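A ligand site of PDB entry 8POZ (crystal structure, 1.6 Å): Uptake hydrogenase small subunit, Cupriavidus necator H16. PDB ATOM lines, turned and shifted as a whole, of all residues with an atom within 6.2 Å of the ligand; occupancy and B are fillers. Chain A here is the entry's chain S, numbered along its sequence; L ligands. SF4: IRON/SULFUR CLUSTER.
An iron atom (FE1) of the ligand is bound by a ring nitrogen (ND1) of His 187 (2.1 Å). An iron atom (FE3) of the ligand is bound by the side-chain sulfur (SG) of Cys 190, 2.3 Å away. FE2 of the ligand is bound by SG of Cys 221 (2.3 Å). SG of Cys 215 binds FE4 of the ligand (2.3 Å). S2 of the ligand lies close to N of Arg 193, at 3.6 Å. N of Leu 216 lies close to S1 of the ligand.
SG of Cys 221 sits close to N of Cys 249 (3.5 Å). The backbone carbonyl oxygen (O) of Ile 243 is in hydrogen-bond range of the guanidinium group (NH2) of Arg 192, 2.9 Å away. N of His 187 lies within hydrogen-bond range of O of Gly 223 (3.3 Å). The guanidinium group of Arg 192 sits at hydrogen-bond distance from the backbone carbonyl oxygen of Phe 214. N of Cys 221 lies within hydrogen-bond range of O of Leu 216. SG of Cys 215 sits close to N of Tyr 217 (3.3 Å). N of Arg 192 sits close to SG of Cys 190 (3.5 Å). The guanidinium group (NE) of Arg 192 is in hydrogen-bond range of the side-chain hydroxyl (OH) of Tyr 191, 3.1 Å away.
Merely in contact with the ligand: Arg 192 (3.8 Å), Phe 196 (3.9 Å), Tyr 217 (3.8 Å), Gly 223 (3.8 Å), Pro 224 (3.8 Å) and Ile 243 (3.7 Å). Of the 22 residues printed, 12 come within 4 Å of the ligand.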
ATOM      1  N   ILE A 186      -7.987 -18.114 -14.174  1.00  0.00           N
ATOM      2  CA  ILE A 186      -7.478 -16.882 -13.559  1.00  0.00           C
ATOM      3  C   ILE A 186      -6.796 -16.020 -14.621  1.00  0.00           C
ATOM      4  O   ILE A 186      -7.035 -14.812 -14.707  1.00  0.00           O
ATOM      5  CB  ILE A 186      -6.456 -17.184 -12.426  1.00  0.00           C
ATOM      6  CG1 ILE A 186      -7.024 -18.142 -11.379  1.00  0.00           C
ATOM      7  CG2 ILE A 186      -5.992 -15.918 -11.734  1.00  0.00           C
ATOM      8  CD1 ILE A 186      -8.361 -17.739 -10.804  1.00  0.00           C
ATOM      9  N   HIS A 187      -5.964 -16.670 -15.416  1.00  0.00           N
ATOM     10  CA  HIS A 187      -5.114 -16.038 -16.447  1.00  0.00           C
ATOM     11  C   HIS A 187      -5.901 -15.360 -17.579  1.00  0.00           C
ATOM     12  O   HIS A 187      -5.376 -14.457 -18.239  1.00  0.00           O
ATOM     13  CB  HIS A 187      -4.189 -17.141 -16.976  1.00  0.00           C
ATOM     14  CG  HIS A 187      -3.110 -16.688 -17.910  1.00  0.00           C
ATOM     15  ND1 HIS A 187      -1.951 -16.085 -17.480  1.00  0.00           N
ATOM     16  CD2 HIS A 187      -2.988 -16.811 -19.256  1.00  0.00           C
ATOM     17  CE1 HIS A 187      -1.173 -15.824 -18.519  1.00  0.00           C
ATOM     18  NE2 HIS A 187      -1.770 -16.269 -19.604  1.00  0.00           N
ATOM     19  N   ASP A 188      -7.150 -15.772 -17.805  1.00  0.00           N
ATOM     20  CA  ASP A 188      -7.983 -15.196 -18.882  1.00  0.00           C
ATOM     21  C   ASP A 188      -8.164 -13.679 -18.736  1.00  0.00           C
ATOM     22  O   ASP A 188      -7.963 -12.955 -19.702  1.00  0.00           O
ATOM     23  CB  ASP A 188      -9.366 -15.861 -18.945  1.00  0.00           C
ATOM     24  CG  ASP A 188      -9.304 -17.322 -19.384  1.00  0.00           C
ATOM     25  OD1 ASP A 188      -8.290 -17.743 -19.987  1.00  0.00           O
ATOM     26  OD2 ASP A 188     -10.289 -18.054 -19.143  1.00  0.00           O
ATOM     27  N   CYS A 190      -6.858 -11.904 -15.776  1.00  0.00           N
ATOM     28  CA  CYS A 190      -5.928 -11.367 -14.792  1.00  0.00           C
ATOM     29  C   CYS A 190      -5.425  -9.996 -15.246  1.00  0.00           C
ATOM     30  O   CYS A 190      -4.956  -9.849 -16.378  1.00  0.00           O
ATOM     31  CB  CYS A 190      -4.748 -12.314 -14.584  1.00  0.00           C
ATOM     32  SG  CYS A 190      -3.536 -11.689 -13.404  1.00  0.00           S
ATOM     33  N   TYR A 191      -5.518  -9.003 -14.359  1.00  0.00           N
ATOM     34  CA  TYR A 191      -5.097  -7.633 -14.695  1.00  0.00           C
ATOM     35  C   TYR A 191      -3.594  -7.503 -14.986  1.00  0.00           C
ATOM     36  O   TYR A 191      -3.170  -6.488 -15.529  1.00  0.00           O
ATOM     37  CB  TYR A 191      -5.507  -6.651 -13.587  1.00  0.00           C
ATOM     38  CG  TYR A 191      -4.543  -6.612 -12.427  1.00  0.00           C
ATOM     39  CD1 TYR A 191      -4.525  -7.637 -11.482  1.00  0.00           C
ATOM     40  CD2 TYR A 191      -3.615  -5.586 -12.296  1.00  0.00           C
ATOM     41  CE1 TYR A 191      -3.628  -7.615 -10.428  1.00  0.00           C
ATOM     42  CE2 TYR A 191      -2.707  -5.555 -11.244  1.00  0.00           C
ATOM     43  CZ  TYR A 191      -2.729  -6.579 -10.311  1.00  0.00           C
ATOM     44  OH  TYR A 191      -1.843  -6.580  -9.273  1.00  0.00           O
ATOM     45  N   ARG A 192      -2.792  -8.500 -14.623  1.00  0.00           N
ATOM     46  CA  ARG A 192      -1.374  -8.527 -14.987  1.00  0.00           C
ATOM     47  C   ARG A 192      -1.089  -9.110 -16.375  1.00  0.00           C
ATOM     48  O   ARG A 192       0.072  -9.179 -16.777  1.00  0.00           O
ATOM     49  CB  ARG A 192      -0.559  -9.285 -13.929  1.00  0.00           C
ATOM     50  CG  ARG A 192      -0.616  -8.614 -12.570  1.00  0.00           C
ATOM     51  CD  ARG A 192       0.512  -9.061 -11.643  1.00  0.00           C
ATOM     52  NE  ARG A 192       0.326  -8.497 -10.311  1.00  0.00           N
ATOM     53  CZ  ARG A 192       1.291  -8.304  -9.398  1.00  0.00           C
ATOM     54  NH1 ARG A 192       2.562  -8.622  -9.649  1.00  0.00           N
ATOM     55  NH2 ARG A 192       0.977  -7.781  -8.221  1.00  0.00           N
ATOM     56  N   ARG A 193      -2.126  -9.524 -17.099  1.00  0.00           N
ATOM     57  CA  ARG A 193      -1.952 -10.112 -18.447  1.00  0.00           C
ATOM     58  C   ARG A 193      -1.153  -9.281 -19.461  1.00  0.00           C
ATOM     59  O   ARG A 193      -0.386  -9.849 -20.225  1.00  0.00           O
ATOM     60  CB  ARG A 193      -3.290 -10.505 -19.081  1.00  0.00           C
ATOM     61  CG  ARG A 193      -3.741 -11.923 -18.780  1.00  0.00           C
ATOM     62  CD  ARG A 193      -2.792 -12.972 -19.348  1.00  0.00           C
ATOM     63  NE  ARG A 193      -2.717 -12.994 -20.812  1.00  0.00           N
ATOM     64  CZ  ARG A 193      -3.577 -13.636 -21.611  1.00  0.00           C
ATOM     65  NH1 ARG A 193      -4.623 -14.302 -21.117  1.00  0.00           N
ATOM     66  NH2 ARG A 193      -3.408 -13.587 -22.926  1.00  0.00           N
ATOM     67  N   PRO A 194      -1.342  -7.951 -19.463  1.00  0.00           N
ATOM     68  CA  PRO A 194      -0.548  -7.157 -20.413  1.00  0.00           C
ATOM     69  C   PRO A 194       0.952  -7.306 -20.192  1.00  0.00           C
ATOM     70  O   PRO A 194       1.720  -7.262 -21.145  1.00  0.00           O
ATOM     71  CB  PRO A 194      -1.019  -5.725 -20.142  1.00  0.00           C
ATOM     72  CG  PRO A 194      -2.386  -5.878 -19.578  1.00  0.00           C
ATOM     73  CD  PRO A 194      -2.301  -7.113 -18.722  1.00  0.00           C
ATOM     74  N   PHE A 196       2.334 -10.174 -18.832  1.00  0.00           N
ATOM     75  CA  PHE A 196       2.590 -11.524 -19.330  1.00  0.00           C
ATOM     76  C   PHE A 196       2.769 -11.514 -20.850  1.00  0.00           C
ATOM     77  O   PHE A 196       3.723 -12.103 -21.372  1.00  0.00           O
ATOM     78  CB  PHE A 196       1.451 -12.483 -18.982  1.00  0.00           C
ATOM     79  CG  PHE A 196       1.623 -13.867 -19.548  1.00  0.00           C
ATOM     80  CD1 PHE A 196       2.313 -14.843 -18.842  1.00  0.00           C
ATOM     81  CD2 PHE A 196       1.113 -14.182 -20.800  1.00  0.00           C
ATOM     82  CE1 PHE A 196       2.471 -16.116 -19.373  1.00  0.00           C
ATOM     83  CE2 PHE A 196       1.274 -15.447 -21.338  1.00  0.00           C
ATOM     84  CZ  PHE A 196       1.953 -16.418 -20.613  1.00  0.00           C
ATOM     85  N   PHE A 201       8.130  -9.853 -16.309  1.00  0.00           N
ATOM     86  CA  PHE A 201       7.965 -10.781 -15.193  1.00  0.00           C
ATOM     87  C   PHE A 201       8.738 -10.394 -13.946  1.00  0.00           C
ATOM     88  O   PHE A 201       9.842  -9.845 -14.033  1.00  0.00           O
ATOM     89  CB  PHE A 201       8.443 -12.181 -15.600  1.00  0.00           C
ATOM     90  CG  PHE A 201       7.722 -12.761 -16.777  1.00  0.00           C
ATOM     91  CD1 PHE A 201       6.425 -13.227 -16.651  1.00  0.00           C
ATOM     92  CD2 PHE A 201       8.363 -12.864 -18.013  1.00  0.00           C
ATOM     93  CE1 PHE A 201       5.757 -13.777 -17.743  1.00  0.00           C
ATOM     94  CE2 PHE A 201       7.695 -13.414 -19.104  1.00  0.00           C
ATOM     95  CZ  PHE A 201       6.399 -13.866 -18.961  1.00  0.00           C
ATOM     96  N   PHE A 214       4.482  -6.513 -12.268  1.00  0.00           N
ATOM     97  CA  PHE A 214       4.740  -7.405 -13.397  1.00  0.00           C
ATOM     98  C   PHE A 214       4.177  -8.805 -13.127  1.00  0.00           C
ATOM     99  O   PHE A 214       3.852  -9.179 -11.983  1.00  0.00           O
ATOM    100  CB  PHE A 214       6.245  -7.461 -13.721  1.00  0.00           C
ATOM    101  CG  PHE A 214       6.767  -6.277 -14.507  1.00  0.00           C
ATOM    102  CD1 PHE A 214       6.029  -5.107 -14.672  1.00  0.00           C
ATOM    103  CD2 PHE A 214       8.050  -6.332 -15.061  1.00  0.00           C
ATOM    104  CE1 PHE A 214       6.539  -4.040 -15.397  1.00  0.00           C
ATOM    105  CE2 PHE A 214       8.555  -5.259 -15.779  1.00  0.00           C
ATOM    106  CZ  PHE A 214       7.800  -4.113 -15.947  1.00  0.00           C
ATOM    107  N   CYS A 215       4.033  -9.570 -14.198  1.00  0.00           N
ATOM    108  CA  CYS A 215       3.430 -10.896 -14.139  1.00  0.00           C
ATOM    109  C   CYS A 215       4.200 -11.825 -13.206  1.00  0.00           C
ATOM    110  O   CYS A 215       5.423 -11.732 -13.118  1.00  0.00           O
ATOM    111  CB  CYS A 215       3.348 -11.497 -15.537  1.00  0.00           C
ATOM    112  SG  CYS A 215       2.830 -13.216 -15.608  1.00  0.00           S
ATOM    113  N   LEU A 216       3.475 -12.705 -12.517  1.00  0.00           N
ATOM    114  CA  LEU A 216       4.049 -13.610 -11.521  1.00  0.00           C
ATOM    115  C   LEU A 216       4.303 -15.039 -12.034  1.00  0.00           C
ATOM    116  O   LEU A 216       4.612 -15.928 -11.233  1.00  0.00           O
ATOM    117  CB  LEU A 216       3.134 -13.645 -10.284  1.00  0.00           C
ATOM    118  CG  LEU A 216       3.053 -12.312  -9.525  1.00  0.00           C
ATOM    119  CD1 LEU A 216       1.877 -12.273  -8.555  1.00  0.00           C
ATOM    120  CD2 LEU A 216       4.339 -12.036  -8.777  1.00  0.00           C
ATOM    121  N   TYR A 217       4.206 -15.249 -13.348  1.00  0.00           N
ATOM    122  CA  TYR A 217       4.401 -16.579 -13.954  1.00  0.00           C
ATOM    123  C   TYR A 217       5.722 -17.218 -13.519  1.00  0.00           C
ATOM    124  O   TYR A 217       5.766 -18.397 -13.171  1.00  0.00           O
ATOM    125  CB  TYR A 217       4.367 -16.482 -15.485  1.00  0.00           C
ATOM    126  CG  TYR A 217       4.414 -17.814 -16.220  1.00  0.00           C
ATOM    127  CD1 TYR A 217       3.242 -18.492 -16.536  1.00  0.00           C
ATOM    128  CD2 TYR A 217       5.620 -18.363 -16.628  1.00  0.00           C
ATOM    129  CE1 TYR A 217       3.275 -19.697 -17.219  1.00  0.00           C
ATOM    130  CE2 TYR A 217       5.666 -19.574 -17.313  1.00  0.00           C
ATOM    131  CZ  TYR A 217       4.490 -20.231 -17.605  1.00  0.00           C
ATOM    132  OH  TYR A 217       4.521 -21.422 -18.288  1.00  0.00           O
ATOM    133  N   CYS A 221       3.240 -18.706 -10.552  1.00  0.00           N
ATOM    134  CA  CYS A 221       1.803 -18.498 -10.696  1.00  0.00           C
ATOM    135  C   CYS A 221       1.139 -19.602 -11.512  1.00  0.00           C
ATOM    136  O   CYS A 221       1.521 -19.856 -12.661  1.00  0.00           O
ATOM    137  CB  CYS A 221       1.491 -17.138 -11.328  1.00  0.00           C
ATOM    138  SG  CYS A 221      -0.294 -16.780 -11.370  1.00  0.00           S
ATOM    139  N   LYS A 222       0.147 -20.245 -10.909  1.00  0.00           N
ATOM    140  CA  LYS A 222      -0.598 -21.315 -11.579  1.00  0.00           C
ATOM    141  C   LYS A 222      -1.925 -20.818 -12.157  1.00  0.00           C
ATOM    142  O   LYS A 222      -2.787 -21.616 -12.551  1.00  0.00           O
ATOM    143  CB  LYS A 222      -0.803 -22.491 -10.618  1.00  0.00           C
ATOM    144  CG  LYS A 222       0.494 -23.107 -10.098  1.00  0.00           C
ATOM    145  CD  LYS A 222       1.492 -23.396 -11.220  1.00  0.00           C
ATOM    146  CE  LYS A 222       2.687 -24.214 -10.771  1.00  0.00           C
ATOM    147  NZ  LYS A 222       3.419 -23.618  -9.620  1.00  0.00           N
ATOM    148  N   GLY A 223      -2.076 -19.494 -12.252  1.00  0.00           N
ATOM    149  CA  GLY A 223      -3.260 -18.909 -12.869  1.00  0.00           C
ATOM    150  C   GLY A 223      -3.578 -19.449 -14.268  1.00  0.00           C
ATOM    151  O   GLY A 223      -4.757 -19.618 -14.596  1.00  0.00           O
ATOM    152  N   PRO A 224      -2.551 -19.707 -15.103  1.00  0.00           N
ATOM    153  CA  PRO A 224      -2.815 -20.267 -16.446  1.00  0.00           C
ATOM    154  C   PRO A 224      -3.479 -21.644 -16.517  1.00  0.00           C
ATOM    155  O   PRO A 224      -4.004 -21.992 -17.574  1.00  0.00           O
ATOM    156  CB  PRO A 224      -1.421 -20.317 -17.086  1.00  0.00           C
ATOM    157  CG  PRO A 224      -0.629 -19.283 -16.364  1.00  0.00           C
ATOM    158  CD  PRO A 224      -1.137 -19.318 -14.947  1.00  0.00           C
ATOM    159  N   PHE A 241      -7.162 -10.051  -4.728  1.00  0.00           N
ATOM    160  CA  PHE A 241      -7.013 -11.501  -4.899  1.00  0.00           C
ATOM    161  C   PHE A 241      -5.526 -11.823  -4.797  1.00  0.00           C
ATOM    162  O   PHE A 241      -4.708 -10.907  -4.771  1.00  0.00           O
ATOM    163  CB  PHE A 241      -7.734 -12.030  -6.158  1.00  0.00           C
ATOM    164  CG  PHE A 241      -7.092 -11.680  -7.470  1.00  0.00           C
ATOM    165  CD1 PHE A 241      -7.002 -10.364  -7.898  1.00  0.00           C
ATOM    166  CD2 PHE A 241      -6.631 -12.684  -8.318  1.00  0.00           C
ATOM    167  CE1 PHE A 241      -6.450 -10.058  -9.132  1.00  0.00           C
ATOM    168  CE2 PHE A 241      -6.066 -12.384  -9.554  1.00  0.00           C
ATOM    169  CZ  PHE A 241      -5.978 -11.061  -9.958  1.00  0.00           C
ATOM    170  N   ILE A 243      -3.012 -12.607  -6.612  1.00  0.00           N
ATOM    171  CA  ILE A 243      -2.104 -11.952  -7.564  1.00  0.00           C
ATOM    172  C   ILE A 243      -2.039 -10.431  -7.366  1.00  0.00           C
ATOM    173  O   ILE A 243      -0.943  -9.855  -7.423  1.00  0.00           O
ATOM    174  CB  ILE A 243      -2.492 -12.337  -9.008  1.00  0.00           C
ATOM    175  CG1 ILE A 243      -2.129 -13.809  -9.234  1.00  0.00           C
ATOM    176  CG2 ILE A 243      -1.823 -11.442 -10.034  1.00  0.00           C
ATOM    177  CD1 ILE A 243      -2.963 -14.509 -10.287  1.00  0.00           C
ATOM    178  N   GLY A 248       1.704 -15.362  -6.534  1.00  0.00           N
ATOM    179  CA  GLY A 248       1.106 -16.137  -7.603  1.00  0.00           C
ATOM    180  C   GLY A 248      -0.046 -17.007  -7.102  1.00  0.00           C
ATOM    181  O   GLY A 248      -0.100 -17.365  -5.917  1.00  0.00           O
ATOM    182  N   CYS A 249      -0.986 -17.303  -7.988  1.00  0.00           N
ATOM    183  CA  CYS A 249      -1.984 -18.338  -7.735  1.00  0.00           C
ATOM    184  C   CYS A 249      -1.232 -19.636  -7.448  1.00  0.00           C
ATOM    185  O   CYS A 249      -0.238 -19.923  -8.120  1.00  0.00           O
ATOM    186  CB  CYS A 249      -2.897 -18.475  -8.966  1.00  0.00           C
ATOM    187  SG  CYS A 249      -4.115 -19.795  -8.904  1.00  0.00           S
HETATM  188 FE1  SF4 L   1      -1.357 -15.117 -15.712  1.00  0.00          FE
HETATM  189 FE2  SF4 L   1      -0.501 -15.326 -13.139  1.00  0.00          FE
HETATM  190 FE3  SF4 L   1      -1.860 -13.140 -14.002  1.00  0.00          FE
HETATM  191 FE4  SF4 L   1       0.691 -13.598 -14.864  1.00  0.00          FE
HETATM  192  S1  SF4 L   1       0.096 -13.125 -12.730  1.00  0.00           S
HETATM  193  S2  SF4 L   1      -1.129 -12.882 -16.120  1.00  0.00           S
HETATM  194  S3  SF4 L   1       0.670 -15.923 -14.964  1.00  0.00           S
HETATM  195  S4  SF4 L   1      -2.653 -15.286 -13.893  1.00  0.00           S
